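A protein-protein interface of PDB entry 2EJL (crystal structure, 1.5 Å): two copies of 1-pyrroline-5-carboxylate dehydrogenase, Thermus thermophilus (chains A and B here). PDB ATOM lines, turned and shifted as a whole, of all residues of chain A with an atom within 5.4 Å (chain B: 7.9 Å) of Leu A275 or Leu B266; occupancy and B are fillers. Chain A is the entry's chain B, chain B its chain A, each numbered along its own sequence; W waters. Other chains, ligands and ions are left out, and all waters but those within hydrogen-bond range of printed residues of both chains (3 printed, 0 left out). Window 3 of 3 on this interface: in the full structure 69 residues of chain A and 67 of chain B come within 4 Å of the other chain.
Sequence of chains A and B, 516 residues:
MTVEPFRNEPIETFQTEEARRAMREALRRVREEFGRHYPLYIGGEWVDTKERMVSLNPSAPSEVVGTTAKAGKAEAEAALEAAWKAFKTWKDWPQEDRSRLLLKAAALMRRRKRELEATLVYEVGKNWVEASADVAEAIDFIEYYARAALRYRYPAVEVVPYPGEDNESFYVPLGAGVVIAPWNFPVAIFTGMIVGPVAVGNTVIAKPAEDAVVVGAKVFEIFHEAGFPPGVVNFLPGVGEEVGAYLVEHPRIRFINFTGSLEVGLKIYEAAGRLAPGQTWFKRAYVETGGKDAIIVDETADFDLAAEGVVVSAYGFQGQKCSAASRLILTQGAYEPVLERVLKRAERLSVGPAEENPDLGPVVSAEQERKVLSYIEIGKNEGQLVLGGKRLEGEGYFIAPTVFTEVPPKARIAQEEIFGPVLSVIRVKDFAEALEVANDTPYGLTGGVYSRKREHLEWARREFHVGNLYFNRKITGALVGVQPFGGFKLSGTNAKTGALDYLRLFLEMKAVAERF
The backbone NH of Glu B270 sits close to the backbone carbonyl oxygen of Gly A273.
The backbone NH (N) of Leu B490 sits at hydrogen-bond distance from the backbone carbonyl oxygen (O) of Thr A280.
OG1 of Thr B289 is in hydrogen-bond range of O of Leu B490, at 2.6 Å.
O of Arg A274 lies within hydrogen-bond range of NE2 of Gln A279 (3.5 Å).
The side-chain amide oxygen (OE1) of Gln A279 is in hydrogen-bond range of the backbone NH (N) of Ala A276, 2.9 Å away.
NE2 of Gln A279 lies within hydrogen-bond range of O of Trp A281, 2.9 Å away.
Among the printed residues, pairs that only touch across the chains: Gly A273 with Tyr B269 (3.6 Å), Arg A274 with Glu B270 (3.9 Å), Leu A275 with Leu B266 (3.9 Å), Leu A275 with Leu B490 (3.9 Å), Gln A279 with Leu B490 (3.9 Å), Thr A280 with Lys B489 (3.1 Å), Trp A281 with Leu B490 (3.6 Å), Phe A282 with Leu B266 (3.8 Å), Phe A282 with Tyr B269 (3.5 Å), Phe A282 with Val B287 (3.9 Å), Phe A282 with Thr B289 (3.7 Å), Phe A282 with Lys B489 (3.7 Å) and Phe A282 with Leu B490 (3.9 Å).
Of the printed residues of chain B, Gly A273 touches Tyr B269 and Glu B270.
Of the printed residues of chain B, Thr A280 touches Lys B489 (3.1 Å) and Leu B490 (3.5 Å).
Of the printed residues of chain B, Phe A282 touches Leu B266 (3.8 Å), Tyr B269 (3.5 Å), Val B287 (3.9 Å), Thr B289 (3.7 Å), Lys B489 (3.7 Å) and Leu B490 (3.9 Å).
Phe B258 touches none of the printed residues of chain A.
Leu B266 touches just these residues of chain A: Leu A275 (3.9 Å) and Phe A282 (3.8 Å).
Ala B272 touches none of the printed residues of chain A.
Of the printed residues of chain A, Lys B489 touches Thr A280 (3.1 Å) and Phe A282 (3.7 Å).
The nearest residue of chain A that does not touch Leu B266 is Gly A273 (4.5 Å).
The nearest printed residue of chain B that does not touch Gly A273 is Leu B266 (4.5 Å).
Among the printed residues, no Asp or Glu carboxylate lies within 4 Å of a Lys or Arg side-chain nitrogen of the other chain.
1 position is printed for both chains.
Water W3 bridges the backbone carbonyl oxygen of Gly A273 and the backbone carbonyl oxygen of Leu B266.
Water W2 lies within hydrogen-bond range of O of Lys B489 (2.8 Å) and N of Phe A282 (2.9 Å).
Water W1 bridges the side-chain carboxylate of Glu B270 (2.8 Å) and the backbone NH of Leu A275 (2.9 Å).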
ATOM      1  N   GLY A 273     -19.187 -22.097   9.758  1.00  0.00           N
ATOM      2  CA  GLY A 273     -17.929 -21.367   9.762  1.00  0.00           C
ATOM      3  C   GLY A 273     -16.789 -22.134  10.418  1.00  0.00           C
ATOM      4  O   GLY A 273     -15.618 -21.732  10.291  1.00  0.00           O
ATOM      5  N   ARG A 274     -17.123 -23.222  11.114  1.00  0.00           N
ATOM      6  CA  ARG A 274     -16.149 -24.039  11.863  1.00  0.00           C
ATOM      7  C   ARG A 274     -15.593 -25.209  11.052  1.00  0.00           C
ATOM      8  O   ARG A 274     -16.308 -25.821  10.253  1.00  0.00           O
ATOM      9  CB  ARG A 274     -16.782 -24.606  13.138  1.00  0.00           C
ATOM     10  CG  ARG A 274     -17.291 -23.578  14.127  1.00  0.00           C
ATOM     11  CD  ARG A 274     -17.568 -24.220  15.486  1.00  0.00           C
ATOM     12  NE  ARG A 274     -18.651 -25.198  15.431  1.00  0.00           N
ATOM     13  CZ  ARG A 274     -19.925 -24.933  15.713  1.00  0.00           C
ATOM     14  NH1 ARG A 274     -20.837 -25.901  15.639  1.00  0.00           N
ATOM     15  NH2 ARG A 274     -20.291 -23.703  16.065  1.00  0.00           N
ATOM     16  N   LEU A 275     -14.323 -25.526  11.277  1.00  0.00           N
ATOM     17  CA  LEU A 275     -13.706 -26.711  10.680  1.00  0.00           C
ATOM     18  C   LEU A 275     -13.910 -27.907  11.607  1.00  0.00           C
ATOM     19  O   LEU A 275     -13.228 -28.019  12.631  1.00  0.00           O
ATOM     20  CB  LEU A 275     -12.208 -26.484  10.411  1.00  0.00           C
ATOM     21  CG  LEU A 275     -11.485 -27.548   9.574  1.00  0.00           C
ATOM     22  CD1 LEU A 275     -11.813 -27.433   8.091  1.00  0.00           C
ATOM     23  CD2 LEU A 275     -10.001 -27.414   9.774  1.00  0.00           C
ATOM     24  N   ALA A 276     -14.856 -28.786  11.271  1.00  0.00           N
ATOM     25  CA  ALA A 276     -15.047 -30.012  12.046  1.00  0.00           C
ATOM     26  C   ALA A 276     -13.794 -30.892  11.962  1.00  0.00           C
ATOM     27  O   ALA A 276     -13.044 -30.830  10.985  1.00  0.00           O
ATOM     28  CB  ALA A 276     -16.266 -30.764  11.561  1.00  0.00           C
ATOM     29  N   PRO A 277     -13.547 -31.720  12.986  1.00  0.00           N
ATOM     30  CA  PRO A 277     -12.336 -32.524  12.885  1.00  0.00           C
ATOM     31  C   PRO A 277     -12.299 -33.364  11.605  1.00  0.00           C
ATOM     32  O   PRO A 277     -13.248 -34.100  11.309  1.00  0.00           O
ATOM     33  CB  PRO A 277     -12.388 -33.415  14.136  1.00  0.00           C
ATOM     34  CG  PRO A 277     -13.269 -32.667  15.097  1.00  0.00           C
ATOM     35  CD  PRO A 277     -14.297 -31.984  14.228  1.00  0.00           C
ATOM     36  N   GLN A 279     -12.348 -32.227   8.539  1.00  0.00           N
ATOM     37  CA  GLN A 279     -12.948 -31.499   7.409  1.00  0.00           C
ATOM     38  C   GLN A 279     -11.871 -30.926   6.483  1.00  0.00           C
ATOM     39  O   GLN A 279     -10.863 -30.416   6.947  1.00  0.00           O
ATOM     40  CB  GLN A 279     -13.842 -30.387   7.940  1.00  0.00           C
ATOM     41  CG  GLN A 279     -14.681 -29.608   6.929  1.00  0.00           C
ATOM     42  CD  GLN A 279     -15.595 -28.659   7.666  1.00  0.00           C
ATOM     43  OE1 GLN A 279     -16.214 -29.037   8.672  1.00  0.00           O
ATOM     44  NE2 GLN A 279     -15.656 -27.404   7.214  1.00  0.00           N
ATOM     45  N   THR A 280     -12.089 -31.028   5.178  1.00  0.00           N
ATOM     46  CA  THR A 280     -11.071 -30.584   4.220  1.00  0.00           C
ATOM     47  C   THR A 280     -11.594 -29.512   3.261  1.00  0.00           C
ATOM     48  O   THR A 280     -11.131 -29.399   2.127  1.00  0.00           O
ATOM     49  CB  THR A 280     -10.507 -31.756   3.407  1.00  0.00           C
ATOM     50  OG1 THR A 280     -11.600 -32.477   2.826  1.00  0.00           O
ATOM     51  CG2 THR A 280      -9.663 -32.694   4.287  1.00  0.00           C
ATOM     52  N   TRP A 281     -12.551 -28.718   3.726  1.00  0.00           N
ATOM     53  CA  TRP A 281     -13.075 -27.590   2.947  1.00  0.00           C
ATOM     54  C   TRP A 281     -13.702 -26.524   3.820  1.00  0.00           C
ATOM     55  O   TRP A 281     -13.965 -26.732   5.017  1.00  0.00           O
ATOM     56  CB  TRP A 281     -14.090 -28.026   1.890  1.00  0.00           C
ATOM     57  CG  TRP A 281     -15.211 -28.880   2.431  1.00  0.00           C
ATOM     58  CD1 TRP A 281     -16.183 -28.506   3.323  1.00  0.00           C
ATOM     59  CD2 TRP A 281     -15.463 -30.245   2.098  1.00  0.00           C
ATOM     60  NE1 TRP A 281     -17.021 -29.572   3.572  1.00  0.00           N
ATOM     61  CE2 TRP A 281     -16.607 -30.646   2.822  1.00  0.00           C
ATOM     62  CE3 TRP A 281     -14.838 -31.169   1.241  1.00  0.00           C
ATOM     63  CZ2 TRP A 281     -17.131 -31.944   2.726  1.00  0.00           C
ATOM     64  CZ3 TRP A 281     -15.352 -32.456   1.149  1.00  0.00           C
ATOM     65  CH2 TRP A 281     -16.489 -32.830   1.878  1.00  0.00           C
ATOM     66  N   PHE A 282     -13.933 -25.368   3.207  1.00  0.00           N
ATOM     67  CA  PHE A 282     -14.723 -24.304   3.825  1.00  0.00           C
ATOM     68  C   PHE A 282     -16.180 -24.515   3.442  1.00  0.00           C
ATOM     69  O   PHE A 282     -16.524 -24.447   2.254  1.00  0.00           O
ATOM     70  CB  PHE A 282     -14.211 -22.923   3.378  1.00  0.00           C
ATOM     71  CG  PHE A 282     -12.851 -22.585   3.918  1.00  0.00           C
ATOM     72  CD1 PHE A 282     -11.697 -22.987   3.240  1.00  0.00           C
ATOM     73  CD2 PHE A 282     -12.720 -21.891   5.118  1.00  0.00           C
ATOM     74  CE1 PHE A 282     -10.429 -22.709   3.761  1.00  0.00           C
ATOM     75  CE2 PHE A 282     -11.456 -21.590   5.635  1.00  0.00           C
ATOM     76  CZ  PHE A 282     -10.314 -21.993   4.965  1.00  0.00           C
ATOM     77  N   PHE B 258      -9.504 -11.888   2.533  1.00  0.00           N
ATOM     78  CA  PHE B 258      -8.236 -12.316   3.154  1.00  0.00           C
ATOM     79  C   PHE B 258      -7.454 -13.216   2.225  1.00  0.00           C
ATOM     80  O   PHE B 258      -8.015 -14.129   1.615  1.00  0.00           O
ATOM     81  CB  PHE B 258      -8.509 -13.063   4.459  1.00  0.00           C
ATOM     82  CG  PHE B 258      -7.317 -13.808   5.013  1.00  0.00           C
ATOM     83  CD1 PHE B 258      -6.345 -13.134   5.741  1.00  0.00           C
ATOM     84  CD2 PHE B 258      -7.166 -15.185   4.802  1.00  0.00           C
ATOM     85  CE1 PHE B 258      -5.246 -13.818   6.268  1.00  0.00           C
ATOM     86  CE2 PHE B 258      -6.062 -15.876   5.318  1.00  0.00           C
ATOM     87  CZ  PHE B 258      -5.109 -15.192   6.066  1.00  0.00           C
ATOM     88  N   SER B 261      -2.172 -17.313   5.383  1.00  0.00           N
ATOM     89  CA  SER B 261      -2.003 -18.685   5.851  1.00  0.00           C
ATOM     90  C   SER B 261      -3.337 -19.323   6.213  1.00  0.00           C
ATOM     91  O   SER B 261      -4.308 -18.638   6.555  1.00  0.00           O
ATOM     92  CB  SER B 261      -1.081 -18.755   7.063  1.00  0.00           C
ATOM     93  OG  SER B 261      -1.777 -18.314   8.203  1.00  0.00           O
ATOM     94  N   LEU B 262      -3.359 -20.648   6.133  1.00  0.00           N
ATOM     95  CA  LEU B 262      -4.541 -21.432   6.481  1.00  0.00           C
ATOM     96  C   LEU B 262      -4.938 -21.223   7.935  1.00  0.00           C
ATOM     97  O   LEU B 262      -6.114 -21.109   8.249  1.00  0.00           O
ATOM     98  CB  LEU B 262      -4.311 -22.921   6.202  1.00  0.00           C
ATOM     99  CG  LEU B 262      -5.439 -23.898   6.554  1.00  0.00           C
ATOM    100  CD1 LEU B 262      -6.706 -23.533   5.816  1.00  0.00           C
ATOM    101  CD2 LEU B 262      -5.024 -25.327   6.267  1.00  0.00           C
ATOM    102  N   GLU B 263      -3.950 -21.180   8.819  1.00  0.00           N
ATOM    103  CA  GLU B 263      -4.251 -21.017  10.231  1.00  0.00           C
ATOM    104  C   GLU B 263      -5.048 -19.738  10.514  1.00  0.00           C
ATOM    105  O   GLU B 263      -6.016 -19.766  11.262  1.00  0.00           O
ATOM    106  CB  GLU B 263      -2.962 -21.096  11.059  1.00  0.00           C
ATOM    107  CG  GLU B 263      -3.003 -20.320  12.357  1.00  0.00           C
ATOM    108  CD  GLU B 263      -1.747 -20.494  13.187  1.00  0.00           C
ATOM    109  OE1 GLU B 263      -0.664 -20.748  12.603  1.00  0.00           O
ATOM    110  OE2 GLU B 263      -1.846 -20.380  14.431  1.00  0.00           O
ATOM    111  N   VAL B 264      -4.642 -18.627   9.903  1.00  0.00           N
ATOM    112  CA  VAL B 264      -5.376 -17.376  10.045  1.00  0.00           C
ATOM    113  C   VAL B 264      -6.727 -17.418   9.299  1.00  0.00           C
ATOM    114  O   VAL B 264      -7.768 -16.969   9.816  1.00  0.00           O
ATOM    115  CB  VAL B 264      -4.511 -16.172   9.609  1.00  0.00           C
ATOM    116  CG1 VAL B 264      -5.280 -14.872   9.744  1.00  0.00           C
ATOM    117  CG2 VAL B 264      -3.266 -16.117  10.482  1.00  0.00           C
ATOM    118  N   GLY B 265      -6.707 -17.965   8.086  1.00  0.00           N
ATOM    119  CA  GLY B 265      -7.934 -18.120   7.309  1.00  0.00           C
ATOM    120  C   GLY B 265      -9.039 -18.886   8.025  1.00  0.00           C
ATOM    121  O   GLY B 265     -10.214 -18.499   7.960  1.00  0.00           O
ATOM    122  N   LEU B 266      -8.667 -19.969   8.704  1.00  0.00           N
ATOM    123  CA  LEU B 266      -9.640 -20.745   9.483  1.00  0.00           C
ATOM    124  C   LEU B 266     -10.267 -19.902  10.589  1.00  0.00           C
ATOM    125  O   LEU B 266     -11.489 -19.931  10.799  1.00  0.00           O
ATOM    126  CB  LEU B 266      -8.996 -22.009  10.062  1.00  0.00           C
ATOM    127  CG  LEU B 266      -8.644 -23.095   9.032  1.00  0.00           C
ATOM    128  CD1 LEU B 266      -7.793 -24.193   9.665  1.00  0.00           C
ATOM    129  CD2 LEU B 266      -9.899 -23.711   8.428  1.00  0.00           C
ATOM    130  N   LYS B 267      -9.420 -19.173  11.314  1.00  0.00           N
ATOM    131  CA  LYS B 267      -9.892 -18.252  12.351  1.00  0.00           C
ATOM    132  C   LYS B 267     -10.824 -17.174  11.803  1.00  0.00           C
ATOM    133  O   LYS B 267     -11.866 -16.900  12.400  1.00  0.00           O
ATOM    134  CB  LYS B 267      -8.728 -17.622  13.121  1.00  0.00           C
ATOM    135  CG  LYS B 267      -7.951 -18.600  13.980  1.00  0.00           C
ATOM    136  CD  LYS B 267      -6.725 -17.929  14.583  1.00  0.00           C
ATOM    137  CE  LYS B 267      -5.877 -18.934  15.350  1.00  0.00           C
ATOM    138  NZ  LYS B 267      -4.558 -18.345  15.740  1.00  0.00           N
ATOM    139  N   ILE B 268     -10.467 -16.577  10.666  1.00  0.00           N
ATOM    140  CA  ILE B 268     -11.305 -15.543  10.054  1.00  0.00           C
ATOM    141  C   ILE B 268     -12.671 -16.096   9.644  1.00  0.00           C
ATOM    142  O   ILE B 268     -13.708 -15.480   9.893  1.00  0.00           O
ATOM    143  CB  ILE B 268     -10.598 -14.861   8.864  1.00  0.00           C
ATOM    144  CG1 ILE B 268      -9.453 -13.972   9.382  1.00  0.00           C
ATOM    145  CG2 ILE B 268     -11.591 -14.052   8.027  1.00  0.00           C
ATOM    146  CD1 ILE B 268      -8.593 -13.365   8.282  1.00  0.00           C
ATOM    147  N   TYR B 269     -12.671 -17.282   9.043  1.00  0.00           N
ATOM    148  CA  TYR B 269     -13.922 -17.844   8.549  1.00  0.00           C
ATOM    149  C   TYR B 269     -14.849 -18.199   9.710  1.00  0.00           C
ATOM    150  O   TYR B 269     -16.070 -18.021   9.616  1.00  0.00           O
ATOM    151  CB  TYR B 269     -13.643 -19.085   7.713  1.00  0.00           C
ATOM    152  CG  TYR B 269     -14.728 -19.424   6.720  1.00  0.00           C
ATOM    153  CD1 TYR B 269     -15.513 -20.586   6.870  1.00  0.00           C
ATOM    154  CD2 TYR B 269     -14.950 -18.613   5.608  1.00  0.00           C
ATOM    155  CE1 TYR B 269     -16.484 -20.924   5.930  1.00  0.00           C
ATOM    156  CE2 TYR B 269     -15.907 -18.935   4.663  1.00  0.00           C
ATOM    157  CZ  TYR B 269     -16.682 -20.082   4.829  1.00  0.00           C
ATOM    158  OH  TYR B 269     -17.639 -20.394   3.879  1.00  0.00           O
ATOM    159  N   GLU B 270     -14.271 -18.725  10.792  1.00  0.00           N
ATOM    160  CA  GLU B 270     -15.050 -19.067  11.973  1.00  0.00           C
ATOM    161  C   GLU B 270     -15.645 -17.806  12.618  1.00  0.00           C
ATOM    162  O   GLU B 270     -16.830 -17.773  12.966  1.00  0.00           O
ATOM    163  CB  GLU B 270     -14.199 -19.860  12.972  1.00  0.00           C
ATOM    164  CG  GLU B 270     -14.984 -20.251  14.211  1.00  0.00           C
ATOM    165  CD  GLU B 270     -14.287 -21.271  15.087  1.00  0.00           C
ATOM    166  OE1 GLU B 270     -13.323 -21.926  14.638  1.00  0.00           O
ATOM    167  OE2 GLU B 270     -14.737 -21.437  16.236  1.00  0.00           O
ATOM    168  N   ALA B 271     -14.836 -16.753  12.736  1.00  0.00           N
ATOM    169  CA  ALA B 271     -15.303 -15.494  13.323  1.00  0.00           C
ATOM    170  C   ALA B 271     -16.399 -14.835  12.460  1.00  0.00           C
ATOM    171  O   ALA B 271     -17.372 -14.271  12.980  1.00  0.00           O
ATOM    172  CB  ALA B 271     -14.126 -14.530  13.534  1.00  0.00           C
ATOM    173  N   ALA B 272     -16.253 -14.929  11.137  1.00  0.00           N
ATOM    174  CA  ALA B 272     -17.211 -14.332  10.213  1.00  0.00           C
ATOM    175  C   ALA B 272     -18.578 -14.992  10.323  1.00  0.00           C
ATOM    176  O   ALA B 272     -19.584 -14.390   9.983  1.00  0.00           O
ATOM    177  CB  ALA B 272     -16.689 -14.424   8.773  1.00  0.00           C
ATOM    178  N   ARG B 274     -20.008 -15.829  13.109  1.00  0.00           N
ATOM    179  CA  ARG B 274     -20.640 -15.385  14.353  1.00  0.00           C
ATOM    180  C   ARG B 274     -21.372 -14.057  14.196  1.00  0.00           C
ATOM    181  O   ARG B 274     -20.951 -13.169  13.443  1.00  0.00           O
ATOM    182  CB  ARG B 274     -19.605 -15.270  15.485  1.00  0.00           C
ATOM    183  CG  ARG B 274     -18.856 -16.567  15.783  1.00  0.00           C
ATOM    184  CD  ARG B 274     -18.046 -16.500  17.087  1.00  0.00           C
ATOM    185  NE  ARG B 274     -17.119 -15.369  17.099  1.00  0.00           N
ATOM    186  CZ  ARG B 274     -15.805 -15.448  16.899  1.00  0.00           C
ATOM    187  NH1 ARG B 274     -15.074 -14.343  16.923  1.00  0.00           N
ATOM    188  NH2 ARG B 274     -15.218 -16.619  16.668  1.00  0.00           N
ATOM    189  N   VAL B 287     -11.656 -16.117   1.493  1.00  0.00           N
ATOM    190  CA  VAL B 287     -10.323 -16.471   1.956  1.00  0.00           C
ATOM    191  C   VAL B 287      -9.573 -17.290   0.906  1.00  0.00           C
ATOM    192  O   VAL B 287     -10.144 -18.197   0.270  1.00  0.00           O
ATOM    193  CB  VAL B 287     -10.335 -17.205   3.342  1.00  0.00           C
ATOM    194  CG1 VAL B 287     -11.072 -16.383   4.414  1.00  0.00           C
ATOM    195  CG2 VAL B 287     -10.936 -18.602   3.251  1.00  0.00           C
ATOM    196  N   THR B 289      -6.068 -19.434   1.008  1.00  0.00           N
ATOM    197  CA  THR B 289      -5.316 -19.958   2.148  1.00  0.00           C
ATOM    198  C   THR B 289      -4.161 -20.900   1.804  1.00  0.00           C
ATOM    199  O   THR B 289      -3.798 -21.757   2.613  1.00  0.00           O
ATOM    200  CB  THR B 289      -6.269 -20.658   3.130  1.00  0.00           C
ATOM    201  OG1 THR B 289      -7.190 -21.469   2.388  1.00  0.00           O
ATOM    202  CG2 THR B 289      -7.047 -19.613   3.923  1.00  0.00           C
ATOM    203  N   LYS B 489     -11.001 -26.933  -1.601  1.00  0.00           N
ATOM    204  CA  LYS B 489     -10.614 -27.543  -0.333  1.00  0.00           C
ATOM    205  C   LYS B 489      -9.996 -26.496   0.592  1.00  0.00           C
ATOM    206  O   LYS B 489     -10.496 -25.353   0.648  1.00  0.00           O
ATOM    207  CB  LYS B 489      -9.712 -28.768  -0.599  1.00  0.00           C
ATOM    208  CG  LYS B 489     -10.462 -29.892  -1.332  1.00  0.00           C
ATOM    209  CD  LYS B 489      -9.509 -30.845  -2.024  1.00  0.00           C
ATOM    210  CE  LYS B 489      -8.583 -31.511  -1.029  1.00  0.00           C
ATOM    211  NZ  LYS B 489      -7.631 -32.436  -1.772  1.00  0.00           N
ATOM    212  N   LEU B 490      -8.940 -26.853   1.329  1.00  0.00           N
ATOM    213  CA  LEU B 490      -8.408 -25.877   2.280  1.00  0.00           C
ATOM    214  C   LEU B 490      -7.515 -24.804   1.655  1.00  0.00           C
ATOM    215  O   LEU B 490      -6.866 -24.047   2.374  1.00  0.00           O
ATOM    216  CB  LEU B 490      -7.803 -26.514   3.535  1.00  0.00           C
ATOM    217  CG  LEU B 490      -8.828 -27.288   4.371  1.00  0.00           C
ATOM    218  CD1 LEU B 490      -8.158 -27.904   5.605  1.00  0.00           C
ATOM    219  CD2 LEU B 490     -10.013 -26.421   4.783  1.00  0.00           C
HETATM  220  O   HOH W   1     -12.546 -23.527  12.447  1.00  0.00           O
HETATM  221  O   HOH W   2     -13.227 -25.120   0.414  1.00  0.00           O
HETATM  222  O   HOH W   3     -12.969 -22.152   9.998  1.00  0.00           O
